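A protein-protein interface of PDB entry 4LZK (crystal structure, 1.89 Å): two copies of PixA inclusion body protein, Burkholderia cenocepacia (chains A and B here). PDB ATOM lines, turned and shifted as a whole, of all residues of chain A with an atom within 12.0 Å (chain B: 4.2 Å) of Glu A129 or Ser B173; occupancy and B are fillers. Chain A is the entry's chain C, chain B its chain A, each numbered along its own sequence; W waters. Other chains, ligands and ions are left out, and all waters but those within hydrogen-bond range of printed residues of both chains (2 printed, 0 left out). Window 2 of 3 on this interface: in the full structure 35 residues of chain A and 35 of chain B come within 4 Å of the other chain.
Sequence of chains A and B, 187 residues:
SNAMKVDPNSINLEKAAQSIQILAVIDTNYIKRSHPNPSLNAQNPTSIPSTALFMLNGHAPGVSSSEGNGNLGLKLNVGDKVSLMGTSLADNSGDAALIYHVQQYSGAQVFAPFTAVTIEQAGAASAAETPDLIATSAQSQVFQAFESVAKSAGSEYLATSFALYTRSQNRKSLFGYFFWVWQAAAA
O of Ser A126 lies within hydrogen-bond range of OG1 of Thr A130 (2.9 Å).
The backbone carbonyl oxygen (O) of Arg B171 is in hydrogen-bond range of the side-chain hydroxyl (OG) of Ser B168 (3.1 Å).
N of Thr B166 lies within hydrogen-bond range of O of Ser B173 (2.8 Å).
The side-chain hydroxyl (OG) of Ser B168 is in hydrogen-bond range of the side-chain hydroxyl (OG) of Ser B173 (3.5 Å).
OG of Ser A126 is in hydrogen-bond range of OE2 of Glu A129.
Glu A129 touches just these residues of chain B: Tyr B165 (2.6 Å), Ser B173 (3.4 Å), Leu B174 (2.7 Å) and Tyr B177 (3.5 Å).
Ser B173 touches just one residue of chain A: Glu A129.
Of chain A, only Ala A125, Glu A129, Thr A130 and Pro A131 come within 4 Å of Tyr B165.
No residue of chain A comes within 4 Å of Ser B168.
Lys B172 touches three residues of chain A.
Leu B174 touches just one residue of chain A: Glu A129.
Of the printed residues of chain B, Gly A123 touches Lys B172.
Of the printed residues of chain A, Tyr B177 touches Glu A129 (3.5 Å) and Pro A131 (3.2 Å).
Of the printed residues of chain B, Ala A125 touches Tyr B165 (3.6 Å) and Lys B172 (3.5 Å).
Of the printed residues of chain B, Ala A122 touches Arg B171 and Lys B172.
The nearest residue of chain A that does not touch Ser B173 is Ala A125 (4.5 Å).
Among the printed residues, merely in contact across the chains: Ala A122 with Arg B171, Ala A122 with Lys B172, Ala A125 with Tyr B165, Ala A125 with Lys B172, Glu A129 with Ser B173, Glu A129 with Tyr B177, Thr A130 with Tyr B165, Pro A131 with Tyr B165 and Pro A131 with Tyr B177.
Hydrophobic or aromatic side chains of chain A within 4 Å of the printed part of chain B: Ala A122, Ala A125 and Pro A131.
Of the 9 printed residues of chain B, 6 touch a printed residue of chain A.
Hydrophobic or aromatic side chains of chain B within 4 Å of the printed part of chain A: Tyr B165, Leu B174 and Tyr B177.
Among the printed residues, no Asp or Glu carboxylate lies within 4 Å of a Lys or Arg side-chain nitrogen of the other chain.
The side-chain carboxylate of Glu A129 sits at hydrogen-bond distance from the backbone NH of Leu B174 (2.7 Å).
The backbone NH (N) of Lys B172 sits close to the backbone carbonyl oxygen (O) of Gly A123 (3.5 Å).
OH of Tyr B165 sits at hydrogen-bond distance from O of Glu A129, 2.6 Å away.
Water W1 lies within hydrogen-bond range of the side-chain carboxylate of Glu A129 (2.5 Å), the backbone carbonyl oxygen of Lys B172 (2.7 Å) and the backbone NH of Ser A126 (3.1 Å).
Water W2 bridges the side-chain hydroxyl of Tyr B177 (2.8 Å) and the backbone carbonyl oxygen of Ala A128 (2.8 Å).
No position is printed for both chains.
Of the 12 pairs that touch across the chains among the printed residues, none has its exchanged pair printed and touching as well.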
ATOM      1  N   GLN A 121     -32.394   0.916   1.183  1.00  0.00           N
ATOM      2  CA  GLN A 121     -31.784   1.846   0.171  1.00  0.00           C
ATOM      3  C   GLN A 121     -30.304   1.562  -0.175  1.00  0.00           C
ATOM      4  O   GLN A 121     -29.496   1.265   0.685  1.00  0.00           O
ATOM      5  CB  GLN A 121     -31.884   3.325   0.675  1.00  0.00           C
ATOM      6  N   ALA A 122     -29.955   1.708  -1.441  1.00  0.00           N
ATOM      7  CA  ALA A 122     -28.589   1.437  -1.852  1.00  0.00           C
ATOM      8  C   ALA A 122     -27.593   2.478  -1.314  1.00  0.00           C
ATOM      9  O   ALA A 122     -27.970   3.565  -0.922  1.00  0.00           O
ATOM     10  CB  ALA A 122     -28.528   1.372  -3.364  1.00  0.00           C
ATOM     11  N   GLY A 123     -26.319   2.138  -1.311  1.00  0.00           N
ATOM     12  CA  GLY A 123     -25.287   3.127  -1.045  1.00  0.00           C
ATOM     13  C   GLY A 123     -25.273   4.162  -2.182  1.00  0.00           C
ATOM     14  O   GLY A 123     -25.953   4.036  -3.207  1.00  0.00           O
ATOM     15  N   ALA A 124     -24.464   5.180  -2.022  1.00  0.00           N
ATOM     16  CA  ALA A 124     -24.450   6.255  -2.969  1.00  0.00           C
ATOM     17  C   ALA A 124     -23.699   5.861  -4.267  1.00  0.00           C
ATOM     18  O   ALA A 124     -22.973   4.837  -4.347  1.00  0.00           O
ATOM     19  CB  ALA A 124     -23.905   7.498  -2.340  1.00  0.00           C
ATOM     20  N   ALA A 125     -23.918   6.653  -5.305  1.00  0.00           N
ATOM     21  CA  ALA A 125     -23.200   6.468  -6.557  1.00  0.00           C
ATOM     22  C   ALA A 125     -21.774   7.094  -6.388  1.00  0.00           C
ATOM     23  O   ALA A 125     -21.539   7.815  -5.426  1.00  0.00           O
ATOM     24  CB  ALA A 125     -23.997   7.077  -7.680  1.00  0.00           C
ATOM     25  N   SER A 126     -20.821   6.814  -7.269  1.00  0.00           N
ATOM     26  CA  SER A 126     -19.461   7.400  -7.079  1.00  0.00           C
ATOM     27  C   SER A 126     -19.579   8.903  -7.203  1.00  0.00           C
ATOM     28  O   SER A 126     -20.615   9.442  -7.709  1.00  0.00           O
ATOM     29  CB  SER A 126     -18.516   6.870  -8.111  1.00  0.00           C
ATOM     30  OG  SER A 126     -18.912   7.332  -9.411  1.00  0.00           O
ATOM     31  N   ALA A 127     -18.524   9.615  -6.803  1.00  0.00           N
ATOM     32  CA  ALA A 127     -18.547  11.067  -6.844  1.00  0.00           C
ATOM     33  C   ALA A 127     -18.678  11.559  -8.317  1.00  0.00           C
ATOM     34  O   ALA A 127     -19.326  12.597  -8.623  1.00  0.00           O
ATOM     35  CB  ALA A 127     -17.246  11.608  -6.176  1.00  0.00           C
ATOM     36  N   ALA A 128     -18.061  10.788  -9.241  1.00  0.00           N
ATOM     37  CA  ALA A 128     -18.004  11.163 -10.665  1.00  0.00           C
ATOM     38  C   ALA A 128     -19.420  11.181 -11.295  1.00  0.00           C
ATOM     39  O   ALA A 128     -19.641  11.824 -12.336  1.00  0.00           O
ATOM     40  CB  ALA A 128     -17.137  10.153 -11.405  1.00  0.00           C
ATOM     41  N   GLU A 129     -20.298  10.410 -10.671  1.00  0.00           N
ATOM     42  CA  GLU A 129     -21.687  10.188 -11.070  1.00  0.00           C
ATOM     43  C   GLU A 129     -22.679  11.062 -10.230  1.00  0.00           C
ATOM     44  O   GLU A 129     -23.876  10.859 -10.302  1.00  0.00           O
ATOM     45  CB  GLU A 129     -22.021   8.726 -10.830  1.00  0.00           C
ATOM     46  CG  GLU A 129     -21.536   7.748 -11.899  1.00  0.00           C
ATOM     47  CD  GLU A 129     -21.729   6.296 -11.431  1.00  0.00           C
ATOM     48  OE1 GLU A 129     -22.707   5.643 -11.849  1.00  0.00           O
ATOM     49  OE2 GLU A 129     -20.965   5.836 -10.515  1.00  0.00           O
ATOM     50  N   THR A 130     -22.188  11.907  -9.327  1.00  0.00           N
ATOM     51  CA  THR A 130     -23.080  12.668  -8.453  1.00  0.00           C
ATOM     52  C   THR A 130     -22.790  14.154  -8.616  1.00  0.00           C
ATOM     53  O   THR A 130     -21.670  14.612  -8.300  1.00  0.00           O
ATOM     54  CB  THR A 130     -22.931  12.277  -6.962  1.00  0.00           C
ATOM     55  OG1 THR A 130     -23.029  10.854  -6.840  1.00  0.00           O
ATOM     56  CG2 THR A 130     -24.034  12.918  -6.072  1.00  0.00           C
ATOM     57  N   PRO A 131     -23.739  14.915  -9.171  1.00  0.00           N
ATOM     58  CA  PRO A 131     -23.587  16.367  -9.045  1.00  0.00           C
ATOM     59  C   PRO A 131     -23.367  16.825  -7.595  1.00  0.00           C
ATOM     60  O   PRO A 131     -24.060  16.398  -6.678  1.00  0.00           O
ATOM     61  CB  PRO A 131     -24.914  16.909  -9.585  1.00  0.00           C
ATOM     62  CG  PRO A 131     -25.329  15.857 -10.590  1.00  0.00           C
ATOM     63  CD  PRO A 131     -24.856  14.542 -10.077  1.00  0.00           C
ATOM     64  N   ASP A 132     -22.424  17.742  -7.411  1.00  0.00           N
ATOM     65  CA  ASP A 132     -22.220  18.354  -6.097  1.00  0.00           C
ATOM     66  C   ASP A 132     -23.497  19.058  -5.652  1.00  0.00           C
ATOM     67  O   ASP A 132     -23.761  19.135  -4.466  1.00  0.00           O
ATOM     68  CB  ASP A 132     -21.022  19.358  -6.080  1.00  0.00           C
ATOM     69  CG  ASP A 132     -21.183  20.566  -7.028  1.00  0.00           C
ATOM     70  OD1 ASP A 132     -21.892  20.507  -8.071  1.00  0.00           O
ATOM     71  OD2 ASP A 132     -20.509  21.610  -6.741  1.00  0.00           O
ATOM     72  N   LEU A 133     -24.274  19.538  -6.621  1.00  0.00           N
ATOM     73  CA  LEU A 133     -25.533  20.237  -6.337  1.00  0.00           C
ATOM     74  C   LEU A 133     -26.515  19.372  -5.518  1.00  0.00           C
ATOM     75  O   LEU A 133     -27.443  19.913  -4.917  1.00  0.00           O
ATOM     76  CB  LEU A 133     -26.193  20.702  -7.649  1.00  0.00           C
ATOM     77  CG  LEU A 133     -25.556  21.860  -8.418  1.00  0.00           C
ATOM     78  CD1 LEU A 133     -26.243  22.082  -9.771  1.00  0.00           C
ATOM     79  CD2 LEU A 133     -25.546  23.170  -7.609  1.00  0.00           C
ATOM     80  N   ILE A 134     -26.304  18.045  -5.473  1.00  0.00           N
ATOM     81  CA  ILE A 134     -27.224  17.144  -4.778  1.00  0.00           C
ATOM     82  C   ILE A 134     -26.740  16.804  -3.366  1.00  0.00           C
ATOM     83  O   ILE A 134     -25.633  16.324  -3.178  1.00  0.00           O
ATOM     84  CB  ILE A 134     -27.512  15.800  -5.535  1.00  0.00           C
ATOM     85  CG1 ILE A 134     -28.115  16.023  -6.907  1.00  0.00           C
ATOM     86  CG2 ILE A 134     -28.472  14.951  -4.755  1.00  0.00           C
ATOM     87  CD1 ILE A 134     -28.145  14.756  -7.776  1.00  0.00           C
ATOM     88  N   ALA A 135     -27.608  17.059  -2.387  1.00  0.00           N
ATOM     89  CA  ALA A 135     -27.540  16.435  -1.065  1.00  0.00           C
ATOM     90  C   ALA A 135     -28.177  15.005  -1.125  1.00  0.00           C
ATOM     91  O   ALA A 135     -29.360  14.799  -1.586  1.00  0.00           O
ATOM     92  CB  ALA A 135     -28.257  17.331  -0.067  1.00  0.00           C
ATOM     93  N   THR A 136     -27.405  13.983  -0.750  1.00  0.00           N
ATOM     94  CA  THR A 136     -28.043  12.659  -0.555  1.00  0.00           C
ATOM     95  C   THR A 136     -27.446  11.914   0.610  1.00  0.00           C
ATOM     96  O   THR A 136     -26.359  12.218   1.018  1.00  0.00           O
ATOM     97  CB  THR A 136     -27.944  11.735  -1.780  1.00  0.00           C
ATOM     98  OG1 THR A 136     -26.649  11.870  -2.382  1.00  0.00           O
ATOM     99  CG2 THR A 136     -28.926  12.092  -2.781  1.00  0.00           C
ATOM    100  N   TYR B 165     -30.785   7.438 -11.132  1.00  0.00           N
ATOM    101  CA  TYR B 165     -29.886   6.348 -10.746  1.00  0.00           C
ATOM    102  C   TYR B 165     -30.624   5.052 -10.735  1.00  0.00           C
ATOM    103  O   TYR B 165     -31.813   5.031 -10.374  1.00  0.00           O
ATOM    104  CB  TYR B 165     -29.390   6.618  -9.321  1.00  0.00           C
ATOM    105  CG  TYR B 165     -28.498   7.867  -9.313  1.00  0.00           C
ATOM    106  CD1 TYR B 165     -27.142   7.796  -9.654  1.00  0.00           C
ATOM    107  CD2 TYR B 165     -29.053   9.102  -8.999  1.00  0.00           C
ATOM    108  CE1 TYR B 165     -26.355   8.935  -9.625  1.00  0.00           C
ATOM    109  CE2 TYR B 165     -28.327  10.272  -9.054  1.00  0.00           C
ATOM    110  CZ  TYR B 165     -26.943  10.178  -9.320  1.00  0.00           C
ATOM    111  OH  TYR B 165     -26.217  11.324  -9.369  1.00  0.00           O
ATOM    112  N   THR B 166     -29.939   3.962 -11.103  1.00  0.00           N
ATOM    113  CA  THR B 166     -30.506   2.641 -10.936  1.00  0.00           C
ATOM    114  C   THR B 166     -29.736   1.969  -9.835  1.00  0.00           C
ATOM    115  O   THR B 166     -28.635   2.393  -9.422  1.00  0.00           O
ATOM    116  CB  THR B 166     -30.286   1.805 -12.197  1.00  0.00           C
ATOM    117  OG1 THR B 166     -28.918   1.894 -12.497  1.00  0.00           O
ATOM    118  CG2 THR B 166     -31.092   2.356 -13.349  1.00  0.00           C
ATOM    119  N   SER B 168     -28.179  -1.520  -8.373  1.00  0.00           N
ATOM    120  CA  SER B 168     -27.664  -2.821  -8.794  1.00  0.00           C
ATOM    121  C   SER B 168     -26.867  -3.322  -7.598  1.00  0.00           C
ATOM    122  O   SER B 168     -26.001  -2.623  -7.123  1.00  0.00           O
ATOM    123  CB  SER B 168     -26.740  -2.595 -10.005  1.00  0.00           C
ATOM    124  OG  SER B 168     -26.134  -1.269  -9.920  1.00  0.00           O
ATOM    125  N   ARG B 171     -25.867  -1.116  -4.689  1.00  0.00           N
ATOM    126  CA  ARG B 171     -25.160   0.059  -5.124  1.00  0.00           C
ATOM    127  C   ARG B 171     -25.931   0.857  -6.244  1.00  0.00           C
ATOM    128  O   ARG B 171     -26.458   0.282  -7.214  1.00  0.00           O
ATOM    129  CB  ARG B 171     -23.784  -0.348  -5.623  1.00  0.00           C
ATOM    130  N   LYS B 172     -25.928   2.171  -6.110  1.00  0.00           N
ATOM    131  CA  LYS B 172     -26.424   3.085  -7.151  1.00  0.00           C
ATOM    132  C   LYS B 172     -25.471   3.393  -8.304  1.00  0.00           C
ATOM    133  O   LYS B 172     -24.292   3.535  -8.105  1.00  0.00           O
ATOM    134  CB  LYS B 172     -26.981   4.383  -6.511  1.00  0.00           C
ATOM    135  CG  LYS B 172     -28.453   4.199  -6.080  1.00  0.00           C
ATOM    136  CD  LYS B 172     -29.066   5.394  -5.373  1.00  0.00           C
ATOM    137  CE  LYS B 172     -29.002   5.172  -3.879  1.00  0.00           C
ATOM    138  NZ  LYS B 172     -28.912   6.493  -3.233  1.00  0.00           N
ATOM    139  N   SER B 173     -26.033   3.538  -9.498  1.00  0.00           N
ATOM    140  CA  SER B 173     -25.315   3.817 -10.743  1.00  0.00           C
ATOM    141  C   SER B 173     -26.086   4.871 -11.494  1.00  0.00           C
ATOM    142  O   SER B 173     -27.359   4.838 -11.502  1.00  0.00           O
ATOM    143  CB  SER B 173     -25.290   2.568 -11.626  1.00  0.00           C
ATOM    144  OG  SER B 173     -24.492   1.598 -11.019  1.00  0.00           O
ATOM    145  N   LEU B 174     -25.382   5.794 -12.092  1.00  0.00           N
ATOM    146  CA  LEU B 174     -26.043   6.871 -12.859  1.00  0.00           C
ATOM    147  C   LEU B 174     -26.644   6.238 -14.122  1.00  0.00           C
ATOM    148  O   LEU B 174     -26.008   5.464 -14.793  1.00  0.00           O
ATOM    149  CB  LEU B 174     -25.112   7.952 -13.258  1.00  0.00           C
ATOM    150  CG  LEU B 174     -25.620   9.075 -14.162  1.00  0.00           C
ATOM    151  CD1 LEU B 174     -26.578   9.981 -13.432  1.00  0.00           C
ATOM    152  CD2 LEU B 174     -24.398   9.826 -14.727  1.00  0.00           C
ATOM    153  N   PHE B 175     -27.885   6.564 -14.408  1.00  0.00           N
ATOM    154  CA  PHE B 175     -28.525   6.171 -15.639  1.00  0.00           C
ATOM    155  C   PHE B 175     -28.472   7.396 -16.573  1.00  0.00           C
ATOM    156  O   PHE B 175     -28.073   7.261 -17.723  1.00  0.00           O
ATOM    157  CB  PHE B 175     -29.981   5.716 -15.443  1.00  0.00           C
ATOM    158  CG  PHE B 175     -30.614   5.260 -16.724  1.00  0.00           C
ATOM    159  CD1 PHE B 175     -30.487   3.961 -17.137  1.00  0.00           C
ATOM    160  CD2 PHE B 175     -31.350   6.160 -17.517  1.00  0.00           C
ATOM    161  CE1 PHE B 175     -30.994   3.556 -18.376  1.00  0.00           C
ATOM    162  CE2 PHE B 175     -31.899   5.759 -18.728  1.00  0.00           C
ATOM    163  CZ  PHE B 175     -31.711   4.469 -19.143  1.00  0.00           C
ATOM    164  N   TYR B 177     -29.211  12.112 -17.026  1.00  0.00           N
ATOM    165  CA  TYR B 177     -29.609  13.392 -16.489  1.00  0.00           C
ATOM    166  C   TYR B 177     -30.709  13.871 -17.379  1.00  0.00           C
ATOM    167  O   TYR B 177     -30.581  13.793 -18.620  1.00  0.00           O
ATOM    168  CB  TYR B 177     -28.512  14.441 -16.474  1.00  0.00           C
ATOM    169  CG  TYR B 177     -27.332  14.105 -15.568  1.00  0.00           C
ATOM    170  CD1 TYR B 177     -27.471  14.183 -14.194  1.00  0.00           C
ATOM    171  CD2 TYR B 177     -26.171  13.710 -16.068  1.00  0.00           C
ATOM    172  CE1 TYR B 177     -26.452  13.842 -13.368  1.00  0.00           C
ATOM    173  CE2 TYR B 177     -25.067  13.378 -15.228  1.00  0.00           C
ATOM    174  CZ  TYR B 177     -25.235  13.465 -13.871  1.00  0.00           C
ATOM    175  OH  TYR B 177     -24.239  13.181 -12.920  1.00  0.00           O
HETATM  176  O   HOH W   1     -21.792   4.283  -8.745  1.00  0.00           O
HETATM  177  O   HOH W   2     -21.930  12.136 -13.996  1.00  0.00           O
